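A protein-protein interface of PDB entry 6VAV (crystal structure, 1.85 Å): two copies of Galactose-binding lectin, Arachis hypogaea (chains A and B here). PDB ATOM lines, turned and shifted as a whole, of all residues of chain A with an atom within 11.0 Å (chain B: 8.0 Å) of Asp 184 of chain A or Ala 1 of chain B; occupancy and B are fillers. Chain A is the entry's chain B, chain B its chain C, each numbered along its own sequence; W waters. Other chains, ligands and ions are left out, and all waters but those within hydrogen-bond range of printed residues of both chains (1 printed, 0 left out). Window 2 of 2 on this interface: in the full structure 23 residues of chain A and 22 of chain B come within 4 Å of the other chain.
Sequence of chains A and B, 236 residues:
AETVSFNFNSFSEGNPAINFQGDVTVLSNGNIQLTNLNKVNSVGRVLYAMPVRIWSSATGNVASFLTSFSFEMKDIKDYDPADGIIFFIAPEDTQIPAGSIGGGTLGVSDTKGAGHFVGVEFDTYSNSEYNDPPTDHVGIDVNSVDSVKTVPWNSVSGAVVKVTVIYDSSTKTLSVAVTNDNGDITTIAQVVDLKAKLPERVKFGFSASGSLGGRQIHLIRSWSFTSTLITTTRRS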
ATOM      1  N   VAL A 138       2.164  -4.423 -18.521  1.00  0.00           N
ATOM      2  CA  VAL A 138       2.645  -3.926 -17.242  1.00  0.00           C
ATOM      3  C   VAL A 138       4.105  -3.672 -17.498  1.00  0.00           C
ATOM      4  O   VAL A 138       4.764  -4.487 -18.116  1.00  0.00           O
ATOM      5  CB  VAL A 138       2.366  -4.846 -16.019  1.00  0.00           C
ATOM      6  CG1 VAL A 138       2.927  -4.223 -14.738  1.00  0.00           C
ATOM      7  CG2 VAL A 138       0.866  -5.106 -15.869  1.00  0.00           C
ATOM      8  N   VAL A 151       5.694  -6.857 -19.548  1.00  0.00           N
ATOM      9  CA  VAL A 151       5.098  -8.182 -19.577  1.00  0.00           C
ATOM     10  C   VAL A 151       3.704  -7.993 -20.238  1.00  0.00           C
ATOM     11  O   VAL A 151       3.014  -7.047 -19.873  1.00  0.00           O
ATOM     12  CB  VAL A 151       5.062  -8.871 -18.172  1.00  0.00           C
ATOM     13  CG1 VAL A 151       4.200  -8.090 -17.156  1.00  0.00           C
ATOM     14  CG2 VAL A 151       4.617 -10.328 -18.273  1.00  0.00           C
ATOM     15  N   PRO A 152       3.276  -8.862 -21.177  1.00  0.00           N
ATOM     16  CA  PRO A 152       1.928  -8.702 -21.757  1.00  0.00           C
ATOM     17  C   PRO A 152       0.856  -8.841 -20.679  1.00  0.00           C
ATOM     18  O   PRO A 152       1.007  -9.600 -19.702  1.00  0.00           O
ATOM     19  CB  PRO A 152       1.850  -9.844 -22.788  1.00  0.00           C
ATOM     20  CG  PRO A 152       3.262 -10.177 -23.096  1.00  0.00           C
ATOM     21  CD  PRO A 152       3.964 -10.026 -21.775  1.00  0.00           C
ATOM     22  N   TRP A 153      -0.188  -8.030 -20.811  1.00  0.00           N
ATOM     23  CA  TRP A 153      -1.282  -7.994 -19.856  1.00  0.00           C
ATOM     24  C   TRP A 153      -2.546  -7.637 -20.648  1.00  0.00           C
ATOM     25  O   TRP A 153      -2.474  -7.486 -21.873  1.00  0.00           O
ATOM     26  CB  TRP A 153      -0.912  -6.996 -18.731  1.00  0.00           C
ATOM     27  CG  TRP A 153      -1.967  -6.693 -17.708  1.00  0.00           C
ATOM     28  CD1 TRP A 153      -2.476  -7.540 -16.773  1.00  0.00           C
ATOM     29  CD2 TRP A 153      -2.581  -5.414 -17.472  1.00  0.00           C
ATOM     30  NE1 TRP A 153      -3.410  -6.885 -15.999  1.00  0.00           N
ATOM     31  CE2 TRP A 153      -3.489  -5.578 -16.402  1.00  0.00           C
ATOM     32  CE3 TRP A 153      -2.484  -4.153 -18.090  1.00  0.00           C
ATOM     33  CZ2 TRP A 153      -4.275  -4.518 -15.920  1.00  0.00           C
ATOM     34  CZ3 TRP A 153      -3.253  -3.106 -17.606  1.00  0.00           C
ATOM     35  CH2 TRP A 153      -4.140  -3.296 -16.542  1.00  0.00           C
ATOM     36  N   ASN A 154      -3.709  -7.600 -19.991  1.00  0.00           N
ATOM     37  CA  ASN A 154      -4.965  -7.279 -20.640  1.00  0.00           C
ATOM     38  C   ASN A 154      -5.779  -6.383 -19.726  1.00  0.00           C
ATOM     39  O   ASN A 154      -6.143  -6.805 -18.618  1.00  0.00           O
ATOM     40  CB  ASN A 154      -5.733  -8.566 -21.006  1.00  0.00           C
ATOM     41  CG  ASN A 154      -7.077  -8.343 -21.684  1.00  0.00           C
ATOM     42  OD1 ASN A 154      -7.315  -7.338 -22.360  1.00  0.00           O
ATOM     43  ND2 ASN A 154      -7.984  -9.295 -21.530  1.00  0.00           N
ATOM     44  N   VAL A 156      -9.079  -5.029 -18.829  1.00  0.00           N
ATOM     45  CA  VAL A 156     -10.499  -5.307 -19.052  1.00  0.00           C
ATOM     46  C   VAL A 156     -11.323  -4.122 -18.540  1.00  0.00           C
ATOM     47  O   VAL A 156     -11.230  -3.755 -17.366  1.00  0.00           O
ATOM     48  CB  VAL A 156     -10.921  -6.659 -18.401  1.00  0.00           C
ATOM     49  CG1 VAL A 156     -12.424  -6.894 -18.512  1.00  0.00           C
ATOM     50  CG2 VAL A 156     -10.142  -7.835 -19.002  1.00  0.00           C
ATOM     51  N   ALA A 159     -13.245  -3.822 -15.010  1.00  0.00           N
ATOM     52  CA  ALA A 159     -12.729  -4.849 -14.094  1.00  0.00           C
ATOM     53  C   ALA A 159     -11.932  -4.222 -12.947  1.00  0.00           C
ATOM     54  O   ALA A 159     -11.195  -3.260 -13.156  1.00  0.00           O
ATOM     55  CB  ALA A 159     -11.866  -5.851 -14.848  1.00  0.00           C
ATOM     56  N   VAL A 160     -12.086  -4.764 -11.742  1.00  0.00           N
ATOM     57  CA  VAL A 160     -11.313  -4.315 -10.577  1.00  0.00           C
ATOM     58  C   VAL A 160     -10.020  -5.129 -10.591  1.00  0.00           C
ATOM     59  O   VAL A 160     -10.065  -6.360 -10.624  1.00  0.00           O
ATOM     60  CB  VAL A 160     -12.075  -4.398  -9.222  1.00  0.00           C
ATOM     61  CG1 VAL A 160     -11.162  -4.036  -8.044  1.00  0.00           C
ATOM     62  CG2 VAL A 160     -13.295  -3.482  -9.247  1.00  0.00           C
ATOM     63  N   VAL A 161      -8.880  -4.435 -10.638  1.00  0.00           N
ATOM     64  CA  VAL A 161      -7.558  -5.056 -10.683  1.00  0.00           C
ATOM     65  C   VAL A 161      -6.856  -4.863  -9.325  1.00  0.00           C
ATOM     66  O   VAL A 161      -6.831  -3.754  -8.788  1.00  0.00           O
ATOM     67  CB  VAL A 161      -6.709  -4.482 -11.855  1.00  0.00           C
ATOM     68  CG1 VAL A 161      -5.337  -5.164 -11.931  1.00  0.00           C
ATOM     69  CG2 VAL A 161      -7.447  -4.592 -13.191  1.00  0.00           C
ATOM     70  N   LYS A 162      -6.276  -5.946  -8.782  1.00  0.00           N
ATOM     71  CA  LYS A 162      -5.525  -5.928  -7.537  1.00  0.00           C
ATOM     72  C   LYS A 162      -4.038  -6.067  -7.826  1.00  0.00           C
ATOM     73  O   LYS A 162      -3.638  -6.903  -8.634  1.00  0.00           O
ATOM     74  CB  LYS A 162      -5.999  -7.043  -6.566  1.00  0.00           C
ATOM     75  CG  LYS A 162      -7.427  -6.846  -6.056  1.00  0.00           C
ATOM     76  CD  LYS A 162      -7.762  -7.776  -4.894  1.00  0.00           C
ATOM     77  CE  LYS A 162      -8.566  -8.984  -5.324  1.00  0.00           C
ATOM     78  NZ  LYS A 162      -8.853  -9.886  -4.181  1.00  0.00           N
ATOM     79  N   VAL A 163      -3.231  -5.208  -7.212  1.00  0.00           N
ATOM     80  CA  VAL A 163      -1.779  -5.221  -7.379  1.00  0.00           C
ATOM     81  C   VAL A 163      -1.095  -5.329  -6.002  1.00  0.00           C
ATOM     82  O   VAL A 163      -1.521  -4.684  -5.049  1.00  0.00           O
ATOM     83  CB  VAL A 163      -1.256  -3.976  -8.164  1.00  0.00           C
ATOM     84  CG1 VAL A 163       0.259  -4.066  -8.408  1.00  0.00           C
ATOM     85  CG2 VAL A 163      -2.001  -3.791  -9.481  1.00  0.00           C
ATOM     86  N   THR A 164      -0.008  -6.090  -5.943  1.00  0.00           N
ATOM     87  CA  THR A 164       0.854  -6.198  -4.800  1.00  0.00           C
ATOM     88  C   THR A 164       2.274  -5.936  -5.286  1.00  0.00           C
ATOM     89  O   THR A 164       2.699  -6.493  -6.287  1.00  0.00           O
ATOM     90  CB  THR A 164       0.696  -7.555  -4.076  1.00  0.00           C
ATOM     91  OG1 THR A 164      -0.635  -7.626  -3.543  1.00  0.00           O
ATOM     92  CG2 THR A 164       1.688  -7.699  -2.916  1.00  0.00           C
ATOM     93  N   VAL A 176       6.329  -7.333  -8.657  1.00  0.00           N
ATOM     94  CA  VAL A 176       4.931  -6.927  -8.871  1.00  0.00           C
ATOM     95  C   VAL A 176       4.059  -8.139  -9.203  1.00  0.00           C
ATOM     96  O   VAL A 176       4.378  -8.876 -10.124  1.00  0.00           O
ATOM     97  CB  VAL A 176       4.840  -5.867 -10.048  1.00  0.00           C
ATOM     98  CG1 VAL A 176       3.413  -5.337 -10.234  1.00  0.00           C
ATOM     99  CG2 VAL A 176       5.810  -4.703  -9.845  1.00  0.00           C
ATOM    100  N   ALA A 177       2.923  -8.271  -8.529  1.00  0.00           N
ATOM    101  CA  ALA A 177       1.931  -9.304  -8.818  1.00  0.00           C
ATOM    102  C   ALA A 177       0.595  -8.611  -9.112  1.00  0.00           C
ATOM    103  O   ALA A 177       0.134  -7.765  -8.332  1.00  0.00           O
ATOM    104  CB  ALA A 177       1.813 -10.299  -7.659  1.00  0.00           C
ATOM    105  N   VAL A 178       0.025  -8.915 -10.274  1.00  0.00           N
ATOM    106  CA  VAL A 178      -1.207  -8.300 -10.804  1.00  0.00           C
ATOM    107  C   VAL A 178      -2.279  -9.385 -10.931  1.00  0.00           C
ATOM    108  O   VAL A 178      -2.083 -10.377 -11.647  1.00  0.00           O
ATOM    109  CB  VAL A 178      -0.959  -7.555 -12.153  1.00  0.00           C
ATOM    110  CG1 VAL A 178      -2.215  -6.812 -12.629  1.00  0.00           C
ATOM    111  CG2 VAL A 178       0.232  -6.601 -12.071  1.00  0.00           C
ATOM    112  N   THR A 179      -3.391  -9.200 -10.212  1.00  0.00           N
ATOM    113  CA  THR A 179      -4.494 -10.150 -10.172  1.00  0.00           C
ATOM    114  C   THR A 179      -5.606  -9.625 -11.050  1.00  0.00           C
ATOM    115  O   THR A 179      -6.301  -8.651 -10.683  1.00  0.00           O
ATOM    116  CB  THR A 179      -4.933 -10.449  -8.715  1.00  0.00           C
ATOM    117  OG1 THR A 179      -3.801 -10.971  -7.995  1.00  0.00           O
ATOM    118  CG2 THR A 179      -6.058 -11.496  -8.645  1.00  0.00           C
ATOM    119  N   ASN A 180      -5.699 -10.271 -12.254  1.00  0.00           N
ATOM    120  CA  ASN A 180      -6.613 -10.093 -13.395  1.00  0.00           C
ATOM    121  C   ASN A 180      -8.038 -10.589 -13.085  1.00  0.00           C
ATOM    122  O   ASN A 180      -8.241 -11.321 -12.110  1.00  0.00           O
ATOM    123  CB  ASN A 180      -6.079 -10.857 -14.615  1.00  0.00           C
ATOM    124  CG  ASN A 180      -4.642 -10.558 -14.994  1.00  0.00           C
ATOM    125  OD1 ASN A 180      -4.379  -9.752 -15.884  1.00  0.00           O
ATOM    126  ND2 ASN A 180      -3.675 -11.238 -14.373  1.00  0.00           N
ATOM    127  N   ASP A 181      -9.024 -10.205 -13.942  1.00  0.00           N
ATOM    128  CA  ASP A 181     -10.443 -10.557 -13.778  1.00  0.00           C
ATOM    129  C   ASP A 181     -10.707 -12.039 -14.142  1.00  0.00           C
ATOM    130  O   ASP A 181     -11.593 -12.646 -13.548  1.00  0.00           O
ATOM    131  CB  ASP A 181     -11.366  -9.560 -14.537  1.00  0.00           C
ATOM    132  CG  ASP A 181     -12.302 -10.045 -15.637  1.00  0.00           C
ATOM    133  OD1 ASP A 181     -11.852 -10.136 -16.801  1.00  0.00           O
ATOM    134  OD2 ASP A 181     -13.505 -10.233 -15.352  1.00  0.00           O
ATOM    135  N   ASN A 182      -9.931 -12.615 -15.069  1.00  0.00           N
ATOM    136  CA  ASN A 182     -10.083 -14.021 -15.459  1.00  0.00           C
ATOM    137  C   ASN A 182      -9.466 -15.019 -14.403  1.00  0.00           C
ATOM    138  O   ASN A 182      -9.479 -16.230 -14.634  1.00  0.00           O
ATOM    139  CB  ASN A 182      -9.502 -14.262 -16.863  1.00  0.00           C
ATOM    140  CG  ASN A 182      -8.004 -14.476 -16.984  1.00  0.00           C
ATOM    141  OD1 ASN A 182      -7.550 -15.300 -17.782  1.00  0.00           O
ATOM    142  ND2 ASN A 182      -7.200 -13.706 -16.261  1.00  0.00           N
ATOM    143  N   GLY A 183      -8.983 -14.490 -13.272  1.00  0.00           N
ATOM    144  CA  GLY A 183      -8.400 -15.249 -12.168  1.00  0.00           C
ATOM    145  C   GLY A 183      -6.895 -15.480 -12.214  1.00  0.00           C
ATOM    146  O   GLY A 183      -6.286 -15.848 -11.208  1.00  0.00           O
ATOM    147  N   ASP A 184      -6.276 -15.289 -13.390  1.00  0.00           N
ATOM    148  CA  ASP A 184      -4.835 -15.474 -13.563  1.00  0.00           C
ATOM    149  C   ASP A 184      -4.027 -14.373 -12.873  1.00  0.00           C
ATOM    150  O   ASP A 184      -4.525 -13.269 -12.649  1.00  0.00           O
ATOM    151  CB  ASP A 184      -4.465 -15.499 -15.055  1.00  0.00           C
ATOM    152  CG  ASP A 184      -5.062 -16.628 -15.875  1.00  0.00           C
ATOM    153  OD1 ASP A 184      -5.912 -17.376 -15.332  1.00  0.00           O
ATOM    154  OD2 ASP A 184      -4.705 -16.744 -17.076  1.00  0.00           O
ATOM    155  N   ILE A 185      -2.764 -14.685 -12.544  1.00  0.00           N
ATOM    156  CA  ILE A 185      -1.863 -13.682 -12.015  1.00  0.00           C
ATOM    157  C   ILE A 185      -0.819 -13.378 -13.064  1.00  0.00           C
ATOM    158  O   ILE A 185      -0.439 -14.261 -13.843  1.00  0.00           O
ATOM    159  CB  ILE A 185      -1.204 -14.023 -10.649  1.00  0.00           C
ATOM    160  CG1 ILE A 185      -0.697 -15.476 -10.609  1.00  0.00           C
ATOM    161  CG2 ILE A 185      -2.123 -13.673  -9.483  1.00  0.00           C
ATOM    162  CD1 ILE A 185       0.737 -15.585 -10.875  1.00  0.00           C
ATOM    163  N   THR A 186      -0.364 -12.123 -13.086  1.00  0.00           N
ATOM    164  CA  THR A 186       0.687 -11.635 -13.965  1.00  0.00           C
ATOM    165  C   THR A 186       1.780 -11.111 -13.061  1.00  0.00           C
ATOM    166  O   THR A 186       1.488 -10.338 -12.154  1.00  0.00           O
ATOM    167  CB  THR A 186       0.131 -10.528 -14.923  1.00  0.00           C
ATOM    168  OG1 THR A 186      -1.008 -11.029 -15.627  1.00  0.00           O
ATOM    169  CG2 THR A 186       1.178 -10.010 -15.903  1.00  0.00           C
ATOM    170  N   THR A 187       3.028 -11.497 -13.290  1.00  0.00           N
ATOM    171  CA  THR A 187       4.097 -10.950 -12.446  1.00  0.00           C
ATOM    172  C   THR A 187       5.172 -10.303 -13.311  1.00  0.00           C
ATOM    173  O   THR A 187       5.406 -10.715 -14.442  1.00  0.00           O
ATOM    174  CB  THR A 187       4.760 -12.003 -11.508  1.00  0.00           C
ATOM    175  OG1 THR A 187       5.476 -12.963 -12.288  1.00  0.00           O
ATOM    176  CG2 THR A 187       3.794 -12.655 -10.526  1.00  0.00           C
ATOM    177  N   ALA B   1      -3.690 -20.004 -20.362  1.00  0.00           N
ATOM    178  CA  ALA B   1      -2.804 -20.340 -19.250  1.00  0.00           C
ATOM    179  C   ALA B   1      -3.483 -21.252 -18.229  1.00  0.00           C
ATOM    180  O   ALA B   1      -4.712 -21.277 -18.119  1.00  0.00           O
ATOM    181  CB  ALA B   1      -2.321 -19.070 -18.575  1.00  0.00           C
ATOM    182  N   GLU B   2      -2.653 -21.994 -17.479  1.00  0.00           N
ATOM    183  CA  GLU B   2      -3.048 -22.937 -16.448  1.00  0.00           C
ATOM    184  C   GLU B   2      -2.904 -22.264 -15.093  1.00  0.00           C
ATOM    185  O   GLU B   2      -1.793 -21.900 -14.704  1.00  0.00           O
ATOM    186  CB  GLU B   2      -2.170 -24.170 -16.564  1.00  0.00           C
ATOM    187  CG  GLU B   2      -2.562 -25.343 -15.686  1.00  0.00           C
ATOM    188  CD  GLU B   2      -1.747 -26.574 -16.029  1.00  0.00           C
ATOM    189  OE1 GLU B   2      -1.993 -27.167 -17.103  1.00  0.00           O
ATOM    190  OE2 GLU B   2      -0.792 -26.884 -15.284  1.00  0.00           O
ATOM    191  N   THR B   3      -4.037 -22.061 -14.399  1.00  0.00           N
ATOM    192  CA  THR B   3      -4.074 -21.382 -13.105  1.00  0.00           C
ATOM    193  C   THR B   3      -4.643 -22.269 -11.992  1.00  0.00           C
ATOM    194  O   THR B   3      -5.668 -22.930 -12.172  1.00  0.00           O
ATOM    195  CB  THR B   3      -4.861 -20.061 -13.227  1.00  0.00           C
ATOM    196  OG1 THR B   3      -4.108 -19.174 -14.047  1.00  0.00           O
ATOM    197  CG2 THR B   3      -5.140 -19.394 -11.874  1.00  0.00           C
ATOM    198  N   VAL B   4      -3.955 -22.254 -10.830  1.00  0.00           N
ATOM    199  CA  VAL B   4      -4.395 -22.886  -9.597  1.00  0.00           C
ATOM    200  C   VAL B   4      -4.683 -21.750  -8.637  1.00  0.00           C
ATOM    201  O   VAL B   4      -3.813 -20.903  -8.415  1.00  0.00           O
ATOM    202  CB  VAL B   4      -3.399 -23.921  -9.009  1.00  0.00           C
ATOM    203  CG1 VAL B   4      -3.895 -24.477  -7.648  1.00  0.00           C
ATOM    204  CG2 VAL B   4      -3.184 -25.061  -9.995  1.00  0.00           C
ATOM    205  N   SER B   5      -5.889 -21.730  -8.075  1.00  0.00           N
ATOM    206  CA  SER B   5      -6.272 -20.682  -7.153  1.00  0.00           C
ATOM    207  C   SER B   5      -7.103 -21.234  -6.010  1.00  0.00           C
ATOM    208  O   SER B   5      -8.032 -22.010  -6.244  1.00  0.00           O
ATOM    209  CB  SER B   5      -7.038 -19.577  -7.887  1.00  0.00           C
ATOM    210  OG  SER B   5      -6.950 -18.374  -7.146  1.00  0.00           O
ATOM    211  N   ARG B  53       1.262 -27.948 -10.833  1.00  0.00           N
ATOM    212  CA  ARG B  53       2.273 -28.040 -11.887  1.00  0.00           C
ATOM    213  C   ARG B  53       2.978 -26.682 -12.001  1.00  0.00           C
ATOM    214  O   ARG B  53       2.391 -25.724 -12.517  1.00  0.00           O
ATOM    215  CB  ARG B  53       1.623 -28.461 -13.217  1.00  0.00           C
ATOM    216  CG  ARG B  53       2.621 -28.918 -14.279  1.00  0.00           C
ATOM    217  CD  ARG B  53       1.956 -29.620 -15.453  1.00  0.00           C
ATOM    218  NE  ARG B  53       1.244 -28.703 -16.353  1.00  0.00           N
ATOM    219  CZ  ARG B  53       1.438 -28.610 -17.669  1.00  0.00           C
ATOM    220  NH1 ARG B  53       0.734 -27.746 -18.386  1.00  0.00           N
ATOM    221  NH2 ARG B  53       2.340 -29.378 -18.275  1.00  0.00           N
ATOM    222  N   THR B 226      -2.385 -18.222  -5.690  1.00  0.00           N
ATOM    223  CA  THR B 226      -2.645 -18.185  -7.126  1.00  0.00           C
ATOM    224  C   THR B 226      -1.343 -18.414  -7.858  1.00  0.00           C
ATOM    225  O   THR B 226      -0.389 -17.667  -7.672  1.00  0.00           O
ATOM    226  CB  THR B 226      -3.341 -16.896  -7.658  1.00  0.00           C
ATOM    227  OG1 THR B 226      -4.462 -16.542  -6.857  1.00  0.00           O
ATOM    228  CG2 THR B 226      -3.817 -17.051  -9.127  1.00  0.00           C
ATOM    229  N   SER B 227      -1.328 -19.418  -8.717  1.00  0.00           N
ATOM    230  CA  SER B 227      -0.219 -19.700  -9.618  1.00  0.00           C
ATOM    231  C   SER B 227      -0.751 -19.696 -11.019  1.00  0.00           C
ATOM    232  O   SER B 227      -1.884 -20.128 -11.236  1.00  0.00           O
ATOM    233  CB  SER B 227       0.462 -21.041  -9.305  1.00  0.00           C
ATOM    234  OG  SER B 227      -0.395 -22.148  -9.530  1.00  0.00           O
ATOM    235  N   THR B 228       0.044 -19.200 -11.963  1.00  0.00           N
ATOM    236  CA  THR B 228      -0.290 -19.219 -13.374  1.00  0.00           C
ATOM    237  C   THR B 228       0.920 -19.688 -14.171  1.00  0.00           C
ATOM    238  O   THR B 228       2.003 -19.099 -14.094  1.00  0.00           O
ATOM    239  CB  THR B 228      -0.824 -17.858 -13.860  1.00  0.00           C
ATOM    240  OG1 THR B 228      -2.010 -17.529 -13.120  1.00  0.00           O
ATOM    241  CG2 THR B 228      -1.097 -17.838 -15.369  1.00  0.00           C
ATOM    242  N   LEU B 229       0.712 -20.738 -14.945  1.00  0.00           N
ATOM    243  CA  LEU B 229       1.703 -21.316 -15.856  1.00  0.00           C
ATOM    244  C   LEU B 229       1.229 -21.075 -17.329  1.00  0.00           C
ATOM    245  O   LEU B 229       0.079 -21.382 -17.671  1.00  0.00           O
ATOM    246  CB  LEU B 229       1.912 -22.823 -15.534  1.00  0.00           C
ATOM    247  CG  LEU B 229       2.742 -23.662 -16.550  1.00  0.00           C
ATOM    248  CD1 LEU B 229       4.194 -23.194 -16.609  1.00  0.00           C
ATOM    249  CD2 LEU B 229       2.742 -25.140 -16.178  1.00  0.00           C
ATOM    250  N   ILE B 230       2.098 -20.457 -18.161  1.00  0.00           N
ATOM    251  CA  ILE B 230       1.827 -20.198 -19.588  1.00  0.00           C
ATOM    252  C   ILE B 230       1.935 -21.556 -20.319  1.00  0.00           C
ATOM    253  O   ILE B 230       2.932 -22.280 -20.161  1.00  0.00           O
ATOM    254  CB  ILE B 230       2.748 -19.089 -20.185  1.00  0.00           C
ATOM    255  CG1 ILE B 230       2.391 -17.712 -19.601  1.00  0.00           C
ATOM    256  CG2 ILE B 230       2.698 -19.045 -21.746  1.00  0.00           C
ATOM    257  CD1 ILE B 230       3.391 -16.707 -19.797  1.00  0.00           C
ATOM    258  N   THR B 231       0.863 -21.940 -21.032  1.00  0.00           N
ATOM    259  CA  THR B 231       0.787 -23.223 -21.754  1.00  0.00           C
ATOM    260  C   THR B 231       1.044 -23.024 -23.275  1.00  0.00           C
ATOM    261  O   THR B 231       1.212 -24.010 -24.003  1.00  0.00           O
ATOM    262  CB  THR B 231      -0.555 -23.924 -21.466  1.00  0.00           C
ATOM    263  OG1 THR B 231      -1.616 -22.980 -21.585  1.00  0.00           O
ATOM    264  CG2 THR B 231      -0.601 -24.543 -20.076  1.00  0.00           C
ATOM    265  N   THR B 232       1.175 -21.757 -23.728  1.00  0.00           N
ATOM    266  CA  THR B 232       1.537 -21.447 -25.118  1.00  0.00           C
ATOM    267  C   THR B 232       3.035 -21.065 -25.199  1.00  0.00           C
ATOM    268  O   THR B 232       3.901 -21.740 -24.632  1.00  0.00           O
ATOM    269  CB  THR B 232       0.622 -20.366 -25.733  1.00  0.00           C
ATOM    270  OG1 THR B 232       0.951 -20.215 -27.119  1.00  0.00           O
ATOM    271  CG2 THR B 232       0.704 -19.013 -25.009  1.00  0.00           C
HETATM  272  O   HOH W   1      -6.667 -19.743 -16.452  1.00  0.00           O
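The side-chain hydroxyl of Thr 228 of chain B sits at hydrogen-bond distance from the backbone NH of Ile 185 of chain A.
The side-chain hydroxyl of Thr 3 of chain B lies within hydrogen-bond range of the side-chain carboxylate of Asp 184 of chain A, at 2.9 Å.
The side-chain amide oxygen (OD1) of Asn 182 of chain A sits close to the side-chain carboxylate (OD2) of Asp 184 of chain A (3.3 Å).
The side-chain hydroxyl (OG) of Ser 5 of chain B sits at hydrogen-bond distance from the side-chain hydroxyl (OG1) of Thr 226 of chain B, 3.1 Å away.
The side-chain amide nitrogen of Asn 180 of chain A sits at hydrogen-bond distance from the backbone carbonyl oxygen of Asp 184 of chain A (2.8 Å).
OG1 of Thr 3 of chain B sits at hydrogen-bond distance from OG1 of Thr 228 of chain B, at 2.8 Å.
Thr 3 of chain B touches Gly 183 of chain A.
O of Gly 183 of chain A touches CG2 of Thr 226 of chain B, 3.4 Å away.
Asp 184 of chain A touches Ala 1 of chain B (OD2 to CB, 3.7 Å).
Asp 184 of chain A touches Thr 228 of chain B (CA to OG1, 3.5 Å).
Ile 185 of chain A touches Thr 226 of chain B (CG1 to O, 3.7 Å).
Asp 184 of chain A touches just these residues of chain B: Ala 1, Thr 3 and Thr 228.
Ala 1 of chain B touches just one residue of chain A: Asp 184 (3.7 Å).
No residue of chain A comes within 4 Å of Glu 2 of chain B.
Of the printed residues of chain A, Thr 3 of chain B touches Gly 183 (3.8 Å) and Asp 184 (2.9 Å).
Of chain A, only Asp 184 (3.5 Å) and Ile 185 (3.0 Å) come within 4 Å of Thr 228 of chain B.
Of the printed residues of chain B, Ile 185 of chain A touches Thr 226 (3.7 Å) and Thr 228 (3.0 Å).
Of the printed residues of chain A, Thr 226 of chain B touches Gly 183 (3.4 Å) and Ile 185 (3.7 Å).
Val 138 of chain A touches none of the printed residues of chain B.
The nearest residue of chain B that does not touch Asp 184 of chain A is Thr 226 of chain B (4.6 Å).
The nearest printed residue of chain B that does not touch Ile 185 of chain A is Ser 227 of chain B (4.2 Å).
Hydrophobic or aromatic side chains of chain A within 4 Å of the printed part of chain B: Ile 185.
Along chain A the printed residues that touch a printed residue of chain B span positions 183 to 185.
Printed residues of chain B that touch a printed residue of chain A: Ala 1, Thr 3, Thr 226 and Thr 228.
Hydrophobic or aromatic side chains of chain B within 4 Å of the printed part of chain A: Ala 1.
Among the printed residues, no Asp or Glu carboxylate lies within 4 Å of a Lys or Arg side-chain nitrogen of the other chain.
No position is printed for both chains.
Of the 7 pairs that touch across the chains among the printed residues, none has its exchanged pair printed and touching as well.
Water W1 bridges OD1 of Asp 184 of chain A (2.7 Å) and O of Ala 1 of chain B (3.0 Å).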
